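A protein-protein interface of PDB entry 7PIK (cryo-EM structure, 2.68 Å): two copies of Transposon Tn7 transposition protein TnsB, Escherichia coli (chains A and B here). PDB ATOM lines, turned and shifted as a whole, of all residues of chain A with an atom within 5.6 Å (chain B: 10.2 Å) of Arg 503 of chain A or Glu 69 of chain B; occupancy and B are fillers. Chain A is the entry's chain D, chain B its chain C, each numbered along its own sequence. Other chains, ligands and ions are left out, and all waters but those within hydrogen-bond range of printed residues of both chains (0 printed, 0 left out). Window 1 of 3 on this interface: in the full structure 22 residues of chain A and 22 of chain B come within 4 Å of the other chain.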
ATOM      1  N   MET A 367      38.954   0.983  14.777  1.00  0.00           N
ATOM      2  CA  MET A 367      38.401   1.147  13.443  1.00  0.00           C
ATOM      3  C   MET A 367      37.782   2.534  13.288  1.00  0.00           C
ATOM      4  O   MET A 367      37.543   3.252  14.261  1.00  0.00           O
ATOM      5  CB  MET A 367      37.359   0.069  13.148  1.00  0.00           C
ATOM      6  CG  MET A 367      37.918  -1.339  13.075  1.00  0.00           C
ATOM      7  SD  MET A 367      36.750  -2.492  12.326  1.00  0.00           S
ATOM      8  CE  MET A 367      37.422  -4.062  12.855  1.00  0.00           C
ATOM      9  N   HIS A 369      34.746   3.327  11.872  1.00  0.00           N
ATOM     10  CA  HIS A 369      33.325   3.375  12.202  1.00  0.00           C
ATOM     11  C   HIS A 369      33.107   3.415  13.710  1.00  0.00           C
ATOM     12  O   HIS A 369      32.173   4.067  14.191  1.00  0.00           O
ATOM     13  CB  HIS A 369      32.603   2.181  11.577  1.00  0.00           C
ATOM     14  CG  HIS A 369      33.154   0.852  11.992  1.00  0.00           C
ATOM     15  ND1 HIS A 369      32.538   0.050  12.926  1.00  0.00           N
ATOM     16  CD2 HIS A 369      34.261   0.183  11.593  1.00  0.00           C
ATOM     17  CE1 HIS A 369      33.242  -1.055  13.088  1.00  0.00           C
ATOM     18  NE2 HIS A 369      34.292  -1.000  12.290  1.00  0.00           N
ATOM     19  N   GLU A 372      33.765   7.008  14.724  1.00  0.00           N
ATOM     20  CA  GLU A 372      32.665   7.840  14.248  1.00  0.00           C
ATOM     21  C   GLU A 372      31.439   7.699  15.143  1.00  0.00           C
ATOM     22  O   GLU A 372      30.849   8.701  15.572  1.00  0.00           O
ATOM     23  CB  GLU A 372      32.331   7.471  12.800  1.00  0.00           C
ATOM     24  CG  GLU A 372      30.952   7.908  12.324  1.00  0.00           C
ATOM     25  CD  GLU A 372      30.879   9.388  11.990  1.00  0.00           C
ATOM     26  OE1 GLU A 372      31.941  10.045  11.936  1.00  0.00           O
ATOM     27  OE2 GLU A 372      29.758   9.893  11.776  1.00  0.00           O
ATOM     28  N   ALA A 499      26.834  -0.888  17.277  1.00  0.00           N
ATOM     29  CA  ALA A 499      27.699   0.131  16.695  1.00  0.00           C
ATOM     30  C   ALA A 499      29.181  -0.145  16.915  1.00  0.00           C
ATOM     31  O   ALA A 499      30.015   0.455  16.231  1.00  0.00           O
ATOM     32  CB  ALA A 499      27.344   1.503  17.265  1.00  0.00           C
ATOM     33  N   LEU A 501      30.673  -3.393  17.001  1.00  0.00           N
ATOM     34  CA  LEU A 501      31.137  -4.659  16.456  1.00  0.00           C
ATOM     35  C   LEU A 501      31.999  -4.440  15.213  1.00  0.00           C
ATOM     36  O   LEU A 501      31.919  -3.394  14.567  1.00  0.00           O
ATOM     37  CB  LEU A 501      29.948  -5.549  16.110  1.00  0.00           C
ATOM     38  CG  LEU A 501      29.142  -6.173  17.251  1.00  0.00           C
ATOM     39  CD1 LEU A 501      27.992  -6.990  16.697  1.00  0.00           C
ATOM     40  CD2 LEU A 501      30.017  -7.032  18.149  1.00  0.00           C
ATOM     41  N   PRO A 502      32.846  -5.407  14.869  1.00  0.00           N
ATOM     42  CA  PRO A 502      33.584  -5.335  13.604  1.00  0.00           C
ATOM     43  C   PRO A 502      32.715  -5.663  12.394  1.00  0.00           C
ATOM     44  O   PRO A 502      31.684  -6.336  12.484  1.00  0.00           O
ATOM     45  CB  PRO A 502      34.695  -6.377  13.784  1.00  0.00           C
ATOM     46  CG  PRO A 502      34.190  -7.299  14.823  1.00  0.00           C
ATOM     47  CD  PRO A 502      33.354  -6.476  15.744  1.00  0.00           C
ATOM     48  N   ARG A 503      33.174  -5.177  11.239  1.00  0.00           N
ATOM     49  CA  ARG A 503      32.429  -5.237   9.988  1.00  0.00           C
ATOM     50  C   ARG A 503      33.276  -5.853   8.881  1.00  0.00           C
ATOM     51  O   ARG A 503      34.507  -5.860   8.941  1.00  0.00           O
ATOM     52  CB  ARG A 503      31.979  -3.843   9.531  1.00  0.00           C
ATOM     53  CG  ARG A 503      30.938  -3.180  10.392  1.00  0.00           C
ATOM     54  CD  ARG A 503      30.705  -1.772   9.903  1.00  0.00           C
ATOM     55  NE  ARG A 503      29.742  -1.056  10.726  1.00  0.00           N
ATOM     56  CZ  ARG A 503      29.485   0.238  10.617  1.00  0.00           C
ATOM     57  NH1 ARG A 503      30.104   0.993   9.727  1.00  0.00           N
ATOM     58  NH2 ARG A 503      28.584   0.790  11.423  1.00  0.00           N
ATOM     59  N   ARG A 504      32.592  -6.366   7.860  1.00  0.00           N
ATOM     60  CA  ARG A 504      33.255  -6.803   6.638  1.00  0.00           C
ATOM     61  C   ARG A 504      32.289  -6.738   5.461  1.00  0.00           C
ATOM     62  O   ARG A 504      31.064  -6.774   5.628  1.00  0.00           O
ATOM     63  CB  ARG A 504      33.830  -8.217   6.773  1.00  0.00           C
ATOM     64  CG  ARG A 504      34.895  -8.521   5.730  1.00  0.00           C
ATOM     65  CD  ARG A 504      35.360  -9.953   5.773  1.00  0.00           C
ATOM     66  NE  ARG A 504      36.230 -10.266   4.645  1.00  0.00           N
ATOM     67  CZ  ARG A 504      37.510  -9.924   4.564  1.00  0.00           C
ATOM     68  NH1 ARG A 504      38.105  -9.238   5.525  1.00  0.00           N
ATOM     69  NH2 ARG A 504      38.207 -10.277   3.489  1.00  0.00           N
ATOM     70  N   LYS A 505      32.871  -6.638   4.265  1.00  0.00           N
ATOM     71  CA  LYS A 505      32.117  -6.700   3.020  1.00  0.00           C
ATOM     72  C   LYS A 505      31.615  -8.115   2.762  1.00  0.00           C
ATOM     73  O   LYS A 505      32.322  -9.097   3.003  1.00  0.00           O
ATOM     74  CB  LYS A 505      32.985  -6.246   1.849  1.00  0.00           C
ATOM     75  CG  LYS A 505      33.480  -4.814   1.928  1.00  0.00           C
ATOM     76  CD  LYS A 505      32.340  -3.822   1.797  1.00  0.00           C
ATOM     77  CE  LYS A 505      32.856  -2.391   1.796  1.00  0.00           C
ATOM     78  NZ  LYS A 505      31.750  -1.397   1.712  1.00  0.00           N
ATOM     79  N   GLU A 544      27.661  -4.264   3.550  1.00  0.00           N
ATOM     80  CA  GLU A 544      28.516  -4.567   4.686  1.00  0.00           C
ATOM     81  C   GLU A 544      27.702  -5.214   5.795  1.00  0.00           C
ATOM     82  O   GLU A 544      26.486  -5.011   5.901  1.00  0.00           O
ATOM     83  CB  GLU A 544      29.212  -3.307   5.204  1.00  0.00           C
ATOM     84  CG  GLU A 544      30.559  -3.569   5.839  1.00  0.00           C
ATOM     85  CD  GLU A 544      31.430  -2.336   5.874  1.00  0.00           C
ATOM     86  OE1 GLU A 544      30.875  -1.218   5.922  1.00  0.00           O
ATOM     87  OE2 GLU A 544      32.670  -2.482   5.855  1.00  0.00           O
ATOM     88  N   ALA A 545      28.385  -6.014   6.613  1.00  0.00           N
ATOM     89  CA  ALA A 545      27.750  -6.693   7.729  1.00  0.00           C
ATOM     90  C   ALA A 545      28.651  -6.635   8.953  1.00  0.00           C
ATOM     91  O   ALA A 545      29.877  -6.570   8.842  1.00  0.00           O
ATOM     92  CB  ALA A 545      27.419  -8.153   7.389  1.00  0.00           C
ATOM     93  N   ALA A 546      28.023  -6.668  10.123  1.00  0.00           N
ATOM     94  CA  ALA A 546      28.706  -6.710  11.405  1.00  0.00           C
ATOM     95  C   ALA A 546      28.623  -8.116  11.984  1.00  0.00           C
ATOM     96  O   ALA A 546      27.588  -8.789  11.870  1.00  0.00           O
ATOM     97  CB  ALA A 546      28.105  -5.705  12.389  1.00  0.00           C
ATOM     98  N   TYR A 547      29.722  -8.553  12.599  1.00  0.00           N
ATOM     99  CA  TYR A 547      29.822  -9.898  13.145  1.00  0.00           C
ATOM    100  C   TYR A 547      30.480  -9.861  14.517  1.00  0.00           C
ATOM    101  O   TYR A 547      31.262  -8.960  14.828  1.00  0.00           O
ATOM    102  CB  TYR A 547      30.615 -10.840  12.216  1.00  0.00           C
ATOM    103  CG  TYR A 547      32.034 -10.394  11.940  1.00  0.00           C
ATOM    104  CD1 TYR A 547      32.301  -9.398  11.013  1.00  0.00           C
ATOM    105  CD2 TYR A 547      33.106 -10.967  12.610  1.00  0.00           C
ATOM    106  CE1 TYR A 547      33.586  -8.985  10.763  1.00  0.00           C
ATOM    107  CE2 TYR A 547      34.399 -10.558  12.364  1.00  0.00           C
ATOM    108  CZ  TYR A 547      34.633  -9.566  11.440  1.00  0.00           C
ATOM    109  OH  TYR A 547      35.918  -9.151  11.187  1.00  0.00           O
ATOM    110  N   PHE A 558      23.728  -4.414   6.855  1.00  0.00           N
ATOM    111  CA  PHE A 558      23.271  -3.037   6.743  1.00  0.00           C
ATOM    112  C   PHE A 558      22.795  -2.774   5.322  1.00  0.00           C
ATOM    113  O   PHE A 558      23.630  -2.636   4.416  1.00  0.00           O
ATOM    114  CB  PHE A 558      24.387  -2.068   7.123  1.00  0.00           C
ATOM    115  CG  PHE A 558      24.851  -2.205   8.546  1.00  0.00           C
ATOM    116  CD1 PHE A 558      23.992  -1.937   9.597  1.00  0.00           C
ATOM    117  CD2 PHE A 558      26.146  -2.603   8.831  1.00  0.00           C
ATOM    118  CE1 PHE A 558      24.416  -2.065  10.902  1.00  0.00           C
ATOM    119  CE2 PHE A 558      26.575  -2.731  10.134  1.00  0.00           C
ATOM    120  CZ  PHE A 558      25.710  -2.460  11.171  1.00  0.00           C
ATOM    121  N   VAL A 561      23.223   2.616   2.837  1.00  0.00           N
ATOM    122  CA  VAL A 561      24.375   3.350   3.348  1.00  0.00           C
ATOM    123  C   VAL A 561      23.903   4.608   4.065  1.00  0.00           C
ATOM    124  O   VAL A 561      22.858   5.182   3.741  1.00  0.00           O
ATOM    125  CB  VAL A 561      25.345   3.678   2.195  1.00  0.00           C
ATOM    126  CG1 VAL A 561      26.664   4.222   2.726  1.00  0.00           C
ATOM    127  CG2 VAL A 561      25.579   2.446   1.339  1.00  0.00           C
ATOM    128  N   GLY A 562      24.682   5.041   5.056  1.00  0.00           N
ATOM    129  CA  GLY A 562      24.351   6.206   5.847  1.00  0.00           C
ATOM    130  C   GLY A 562      23.429   5.946   7.017  1.00  0.00           C
ATOM    131  O   GLY A 562      23.042   6.901   7.700  1.00  0.00           O
ATOM    132  N   SER A 563      23.066   4.694   7.269  1.00  0.00           N
ATOM    133  CA  SER A 563      22.194   4.341   8.376  1.00  0.00           C
ATOM    134  C   SER A 563      22.711   3.065   9.021  1.00  0.00           C
ATOM    135  O   SER A 563      23.407   2.265   8.392  1.00  0.00           O
ATOM    136  CB  SER A 563      20.744   4.162   7.911  1.00  0.00           C
ATOM    137  OG  SER A 563      19.869   3.990   9.012  1.00  0.00           O
ATOM    138  N   ARG A 564      22.369   2.881  10.297  1.00  0.00           N
ATOM    139  CA  ARG A 564      22.731   1.677  11.032  1.00  0.00           C
ATOM    140  C   ARG A 564      21.524   0.793  11.318  1.00  0.00           C
ATOM    141  O   ARG A 564      21.546   0.008  12.269  1.00  0.00           O
ATOM    142  CB  ARG A 564      23.456   2.035  12.329  1.00  0.00           C
ATOM    143  CG  ARG A 564      24.907   2.429  12.119  1.00  0.00           C
ATOM    144  CD  ARG A 564      25.737   2.238  13.374  1.00  0.00           C
ATOM    145  NE  ARG A 564      25.312   3.121  14.453  1.00  0.00           N
ATOM    146  CZ  ARG A 564      25.753   4.360  14.627  1.00  0.00           C
ATOM    147  NH1 ARG A 564      26.632   4.902  13.802  1.00  0.00           N
ATOM    148  NH2 ARG A 564      25.294   5.071  15.650  1.00  0.00           N
ATOM    149  N   HIS B  64      15.931   8.344  17.136  1.00  0.00           N
ATOM    150  CA  HIS B  64      16.364   7.791  15.858  1.00  0.00           C
ATOM    151  C   HIS B  64      17.681   8.390  15.378  1.00  0.00           C
ATOM    152  O   HIS B  64      18.384   7.753  14.586  1.00  0.00           O
ATOM    153  CB  HIS B  64      15.280   8.014  14.803  1.00  0.00           C
ATOM    154  CG  HIS B  64      14.880   9.448  14.645  1.00  0.00           C
ATOM    155  ND1 HIS B  64      15.533  10.314  13.795  1.00  0.00           N
ATOM    156  CD2 HIS B  64      13.898  10.171  15.235  1.00  0.00           C
ATOM    157  CE1 HIS B  64      14.969  11.507  13.865  1.00  0.00           C
ATOM    158  NE2 HIS B  64      13.976  11.447  14.732  1.00  0.00           N
ATOM    159  N   LEU B  65      18.044   9.578  15.863  1.00  0.00           N
ATOM    160  CA  LEU B  65      19.308  10.196  15.484  1.00  0.00           C
ATOM    161  C   LEU B  65      20.517   9.391  15.938  1.00  0.00           C
ATOM    162  O   LEU B  65      21.641   9.736  15.561  1.00  0.00           O
ATOM    163  CB  LEU B  65      19.388  11.614  16.053  1.00  0.00           C
ATOM    164  CG  LEU B  65      18.315  12.598  15.586  1.00  0.00           C
ATOM    165  CD1 LEU B  65      18.306  13.839  16.464  1.00  0.00           C
ATOM    166  CD2 LEU B  65      18.522  12.969  14.128  1.00  0.00           C
ATOM    167  N   ASP B  66      20.323   8.335  16.733  1.00  0.00           N
ATOM    168  CA  ASP B  66      21.430   7.446  17.062  1.00  0.00           C
ATOM    169  C   ASP B  66      21.820   6.530  15.910  1.00  0.00           C
ATOM    170  O   ASP B  66      22.899   5.930  15.956  1.00  0.00           O
ATOM    171  CB  ASP B  66      21.086   6.597  18.286  1.00  0.00           C
ATOM    172  CG  ASP B  66      21.437   7.285  19.584  1.00  0.00           C
ATOM    173  OD1 ASP B  66      22.363   8.122  19.578  1.00  0.00           O
ATOM    174  OD2 ASP B  66      20.790   6.990  20.610  1.00  0.00           O
ATOM    175  N   LEU B  67      20.978   6.407  14.885  1.00  0.00           N
ATOM    176  CA  LEU B  67      21.245   5.503  13.773  1.00  0.00           C
ATOM    177  C   LEU B  67      21.886   6.188  12.573  1.00  0.00           C
ATOM    178  O   LEU B  67      22.128   5.525  11.560  1.00  0.00           O
ATOM    179  CB  LEU B  67      19.951   4.818  13.332  1.00  0.00           C
ATOM    180  CG  LEU B  67      19.204   4.032  14.407  1.00  0.00           C
ATOM    181  CD1 LEU B  67      17.905   3.484  13.854  1.00  0.00           C
ATOM    182  CD2 LEU B  67      20.076   2.912  14.932  1.00  0.00           C
ATOM    183  N   GLU B  68      22.176   7.483  12.659  1.00  0.00           N
ATOM    184  CA  GLU B  68      22.614   8.255  11.504  1.00  0.00           C
ATOM    185  C   GLU B  68      24.134   8.283  11.416  1.00  0.00           C
ATOM    186  O   GLU B  68      24.817   8.526  12.414  1.00  0.00           O
ATOM    187  CB  GLU B  68      22.072   9.681  11.578  1.00  0.00           C
ATOM    188  CG  GLU B  68      20.586   9.766  11.858  1.00  0.00           C
ATOM    189  CD  GLU B  68      19.746   9.465  10.637  1.00  0.00           C
ATOM    190  OE1 GLU B  68      19.472   8.275  10.378  1.00  0.00           O
ATOM    191  OE2 GLU B  68      19.357  10.422   9.936  1.00  0.00           O
ATOM    192  N   GLU B  69      24.655   8.033  10.217  1.00  0.00           N
ATOM    193  CA  GLU B  69      26.082   8.174   9.925  1.00  0.00           C
ATOM    194  C   GLU B  69      26.224   8.729   8.516  1.00  0.00           C
ATOM    195  O   GLU B  69      26.410   7.981   7.549  1.00  0.00           O
ATOM    196  CB  GLU B  69      26.819   6.842  10.079  1.00  0.00           C
ATOM    197  CG  GLU B  69      26.065   5.630   9.565  1.00  0.00           C
ATOM    198  CD  GLU B  69      26.855   4.349   9.726  1.00  0.00           C
ATOM    199  OE1 GLU B  69      27.901   4.373  10.406  1.00  0.00           O
ATOM    200  OE2 GLU B  69      26.436   3.317   9.166  1.00  0.00           O
ATOM    201  N   PRO B  70      26.130  10.049   8.360  1.00  0.00           N
ATOM    202  CA  PRO B  70      26.180  10.641   7.017  1.00  0.00           C
ATOM    203  C   PRO B  70      27.495  10.342   6.313  1.00  0.00           C
ATOM    204  O   PRO B  70      28.560  10.307   6.930  1.00  0.00           O
ATOM    205  CB  PRO B  70      26.015  12.142   7.286  1.00  0.00           C
ATOM    206  CG  PRO B  70      25.404  12.229   8.640  1.00  0.00           C
ATOM    207  CD  PRO B  70      25.940  11.066   9.407  1.00  0.00           C
ATOM    208  N   SER B  71      27.405  10.124   5.004  1.00  0.00           N
ATOM    209  CA  SER B  71      28.582   9.837   4.202  1.00  0.00           C
ATOM    210  C   SER B  71      29.438  11.088   4.033  1.00  0.00           C
ATOM    211  O   SER B  71      28.961  12.221   4.134  1.00  0.00           O
ATOM    212  CB  SER B  71      28.180   9.294   2.831  1.00  0.00           C
ATOM    213  OG  SER B  71      27.343   8.158   2.953  1.00  0.00           O
ATOM    214  N   VAL B  72      30.727  10.866   3.773  1.00  0.00           N
ATOM    215  CA  VAL B  72      31.628  11.977   3.503  1.00  0.00           C
ATOM    216  C   VAL B  72      31.235  12.643   2.185  1.00  0.00           C
ATOM    217  O   VAL B  72      30.531  12.065   1.351  1.00  0.00           O
ATOM    218  CB  VAL B  72      33.086  11.480   3.482  1.00  0.00           C
ATOM    219  CG1 VAL B  72      34.077  12.630   3.337  1.00  0.00           C
ATOM    220  CG2 VAL B  72      33.385  10.675   4.735  1.00  0.00           C
ATOM    221  N   ASP B  73      31.658  13.901   2.027  1.00  0.00           N
ATOM    222  CA  ASP B  73      31.408  14.725   0.835  1.00  0.00           C
ATOM    223  C   ASP B  73      29.926  14.767   0.457  1.00  0.00           C
ATOM    224  O   ASP B  73      29.568  14.901  -0.715  1.00  0.00           O
ATOM    225  CB  ASP B  73      32.289  14.299  -0.356  1.00  0.00           C
ATOM    226  CG  ASP B  73      31.982  12.902  -0.888  1.00  0.00           C
ATOM    227  OD1 ASP B  73      30.829  12.624  -1.281  1.00  0.00           O
ATOM    228  OD2 ASP B  73      32.912  12.070  -0.912  1.00  0.00           O
ATOM    229  N   SER B  74      29.055  14.688   1.458  1.00  0.00           N
ATOM    230  CA  SER B  74      27.634  14.948   1.293  1.00  0.00           C
ATOM    231  C   SER B  74      27.299  16.277   1.958  1.00  0.00           C
ATOM    232  O   SER B  74      28.087  16.816   2.738  1.00  0.00           O
ATOM    233  CB  SER B  74      26.783  13.816   1.886  1.00  0.00           C
ATOM    234  OG  SER B  74      27.042  13.645   3.268  1.00  0.00           O
ATOM    235  N   SER B  76      24.887  16.945   4.127  1.00  0.00           N
ATOM    236  CA  SER B  76      24.582  16.796   5.546  1.00  0.00           C
ATOM    237  C   SER B  76      25.853  16.778   6.386  1.00  0.00           C
ATOM    238  O   SER B  76      25.932  17.438   7.429  1.00  0.00           O
ATOM    239  CB  SER B  76      23.770  15.521   5.767  1.00  0.00           C
ATOM    240  OG  SER B  76      22.608  15.516   4.959  1.00  0.00           O
ATOM    241  N   PHE B  77      26.863  16.034   5.936  1.00  0.00           N
ATOM    242  CA  PHE B  77      28.110  15.916   6.686  1.00  0.00           C
ATOM    243  C   PHE B  77      28.788  17.274   6.847  1.00  0.00           C
ATOM    244  O   PHE B  77      29.137  17.686   7.963  1.00  0.00           O
ATOM    245  CB  PHE B  77      29.030  14.921   5.974  1.00  0.00           C
ATOM    246  CG  PHE B  77      30.314  14.639   6.698  1.00  0.00           C
ATOM    247  CD1 PHE B  77      30.378  13.640   7.652  1.00  0.00           C
ATOM    248  CD2 PHE B  77      31.462  15.355   6.407  1.00  0.00           C
ATOM    249  CE1 PHE B  77      31.559  13.372   8.315  1.00  0.00           C
ATOM    250  CE2 PHE B  77      32.643  15.093   7.069  1.00  0.00           C
ATOM    251  CZ  PHE B  77      32.691  14.100   8.022  1.00  0.00           C
ATOM    252  N   GLN B  78      28.965  17.990   5.734  1.00  0.00           N
ATOM    253  CA  GLN B  78      29.655  19.274   5.773  1.00  0.00           C
ATOM    254  C   GLN B  78      28.865  20.305   6.567  1.00  0.00           C
ATOM    255  O   GLN B  78      29.443  21.082   7.337  1.00  0.00           O
ATOM    256  CB  GLN B  78      29.910  19.768   4.351  1.00  0.00           C
ATOM    257  CG  GLN B  78      30.629  18.760   3.475  1.00  0.00           C
ATOM    258  CD  GLN B  78      30.728  19.211   2.033  1.00  0.00           C
ATOM    259  OE1 GLN B  78      30.265  20.294   1.676  1.00  0.00           O
ATOM    260  NE2 GLN B  78      31.331  18.379   1.193  1.00  0.00           N
ATOM    261  N   ARG B  80      26.755  19.736   9.033  1.00  0.00           N
ATOM    262  CA  ARG B  80      26.869  19.398  10.447  1.00  0.00           C
ATOM    263  C   ARG B  80      28.209  19.852  11.010  1.00  0.00           C
ATOM    264  O   ARG B  80      28.272  20.454  12.092  1.00  0.00           O
ATOM    265  CB  ARG B  80      26.688  17.893  10.638  1.00  0.00           C
ATOM    266  CG  ARG B  80      26.981  17.406  12.048  1.00  0.00           C
ATOM    267  CD  ARG B  80      26.933  15.895  12.131  1.00  0.00           C
ATOM    268  NE  ARG B  80      28.165  15.287  11.647  1.00  0.00           N
ATOM    269  CZ  ARG B  80      28.348  13.984  11.494  1.00  0.00           C
ATOM    270  NH1 ARG B  80      27.396  13.115  11.786  1.00  0.00           N
ATOM    271  NH2 ARG B  80      29.514  13.541  11.037  1.00  0.00           N
ATOM    272  N   GLU B  81      29.297  19.577  10.282  1.00  0.00           N
ATOM    273  CA  GLU B  81      30.615  19.963  10.777  1.00  0.00           C
ATOM    274  C   GLU B  81      30.736  21.476  10.915  1.00  0.00           C
ATOM    275  O   GLU B  81      31.252  21.974  11.923  1.00  0.00           O
ATOM    276  CB  GLU B  81      31.707  19.416   9.860  1.00  0.00           C
ATOM    277  CG  GLU B  81      31.697  17.904   9.712  1.00  0.00           C
ATOM    278  CD  GLU B  81      31.868  17.179  11.035  1.00  0.00           C
ATOM    279  OE1 GLU B  81      32.621  17.676  11.897  1.00  0.00           O
ATOM    280  OE2 GLU B  81      31.247  16.110  11.211  1.00  0.00           O
ATOM    281  N   ASN B 135      25.203  15.189  16.098  1.00  0.00           N
ATOM    282  CA  ASN B 135      24.180  14.682  15.186  1.00  0.00           C
ATOM    283  C   ASN B 135      22.846  15.401  15.325  1.00  0.00           C
ATOM    284  O   ASN B 135      21.919  15.086  14.574  1.00  0.00           O
ATOM    285  CB  ASN B 135      23.959  13.183  15.398  1.00  0.00           C
ATOM    286  CG  ASN B 135      24.726  12.331  14.414  1.00  0.00           C
ATOM    287  OD1 ASN B 135      25.450  12.840  13.563  1.00  0.00           O
ATOM    288  ND2 ASN B 135      24.559  11.022  14.517  1.00  0.00           N
ATOM    289  N   ILE B 138      22.088  18.199  12.003  1.00  0.00           N
ATOM    290  CA  ILE B 138      21.980  17.673  10.645  1.00  0.00           C
ATOM    291  C   ILE B 138      20.754  18.300   9.991  1.00  0.00           C
ATOM    292  O   ILE B 138      19.671  18.275  10.591  1.00  0.00           O
ATOM    293  CB  ILE B 138      21.885  16.135  10.639  1.00  0.00           C
ATOM    294  CG1 ILE B 138      23.275  15.513  10.780  1.00  0.00           C
ATOM    295  CG2 ILE B 138      21.210  15.630   9.375  1.00  0.00           C
ATOM    296  CD1 ILE B 138      23.256  14.045  11.123  1.00  0.00           C
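NH2 of Arg 564 of chain A is in hydrogen-bond range of O of Asp 66 of chain B. NH2 of Arg 80 of chain B is in salt-bridge range of OE2 of Glu 372 of chain A (3.7 Å). The backbone carbonyl oxygen (O) of Ser 563 of chain A sits close to the side-chain carboxylate (OE2) of Glu 69 of chain B (3.3 Å). The backbone carbonyl oxygen (O) of Gly 562 of chain A sits at hydrogen-bond distance from the backbone NH (N) of Glu 69 of chain B (3.2 Å). The backbone carbonyl oxygen of Leu 67 of chain B sits at hydrogen-bond distance from the backbone NH of Arg 564 of chain A, 2.9 Å away. The side-chain carboxylate (OE1) of Glu 69 of chain B lies within salt-bridge range of the guanidinium group (NH2) of Arg 503 of chain A. OE1 of Glu 69 of chain B is in salt-bridge range of NH1 of Arg 564 of chain A, at 3.7 Å.
Of the 18 printed residues of chain A, 5 touch a printed residue of chain B. Of the 18 printed residues of chain B, 4 touch a printed residue of chain A. Among the printed residues, 8 pairs touch across the chains.
No position is printed for both chains. Of the 8 pairs that touch across the chains among the printed residues, none has its exchanged pair printed and touching as well.
Ser 563 of chain A touches Leu 67 of chain B (CA to O, 3.4 Å).
Of the printed residues of chain B, Arg 503 of chain A touches Glu 69. Printed residues of chain A within 4 Å of Glu 69 of chain B: Arg 503 (3.8 Å), Gly 562 (3.2 Å), Ser 563 (3.3 Å) and Arg 564 (3.4 Å). No residue of chain B comes within 4 Å of Pro 502 of chain A. Gly 562 of chain A touches just one residue of chain B: Glu 69. Printed residues of chain A within 4 Å of Asp 66 of chain B: Arg 564 (2.6 Å). Of the printed residues of chain B, Glu 372 of chain A touches Arg 80. The nearest residue of chain B that does not touch Arg 503 of chain A is Leu 67 of chain B (8.0 Å).
OE2 of Glu 81 of chain B lies within salt-bridge range of NH2 of Arg 80 of chain B (3.1 Å). NH1 of Arg 80 of chain B sits at hydrogen-bond distance from OD1 of Asn 135 of chain B.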
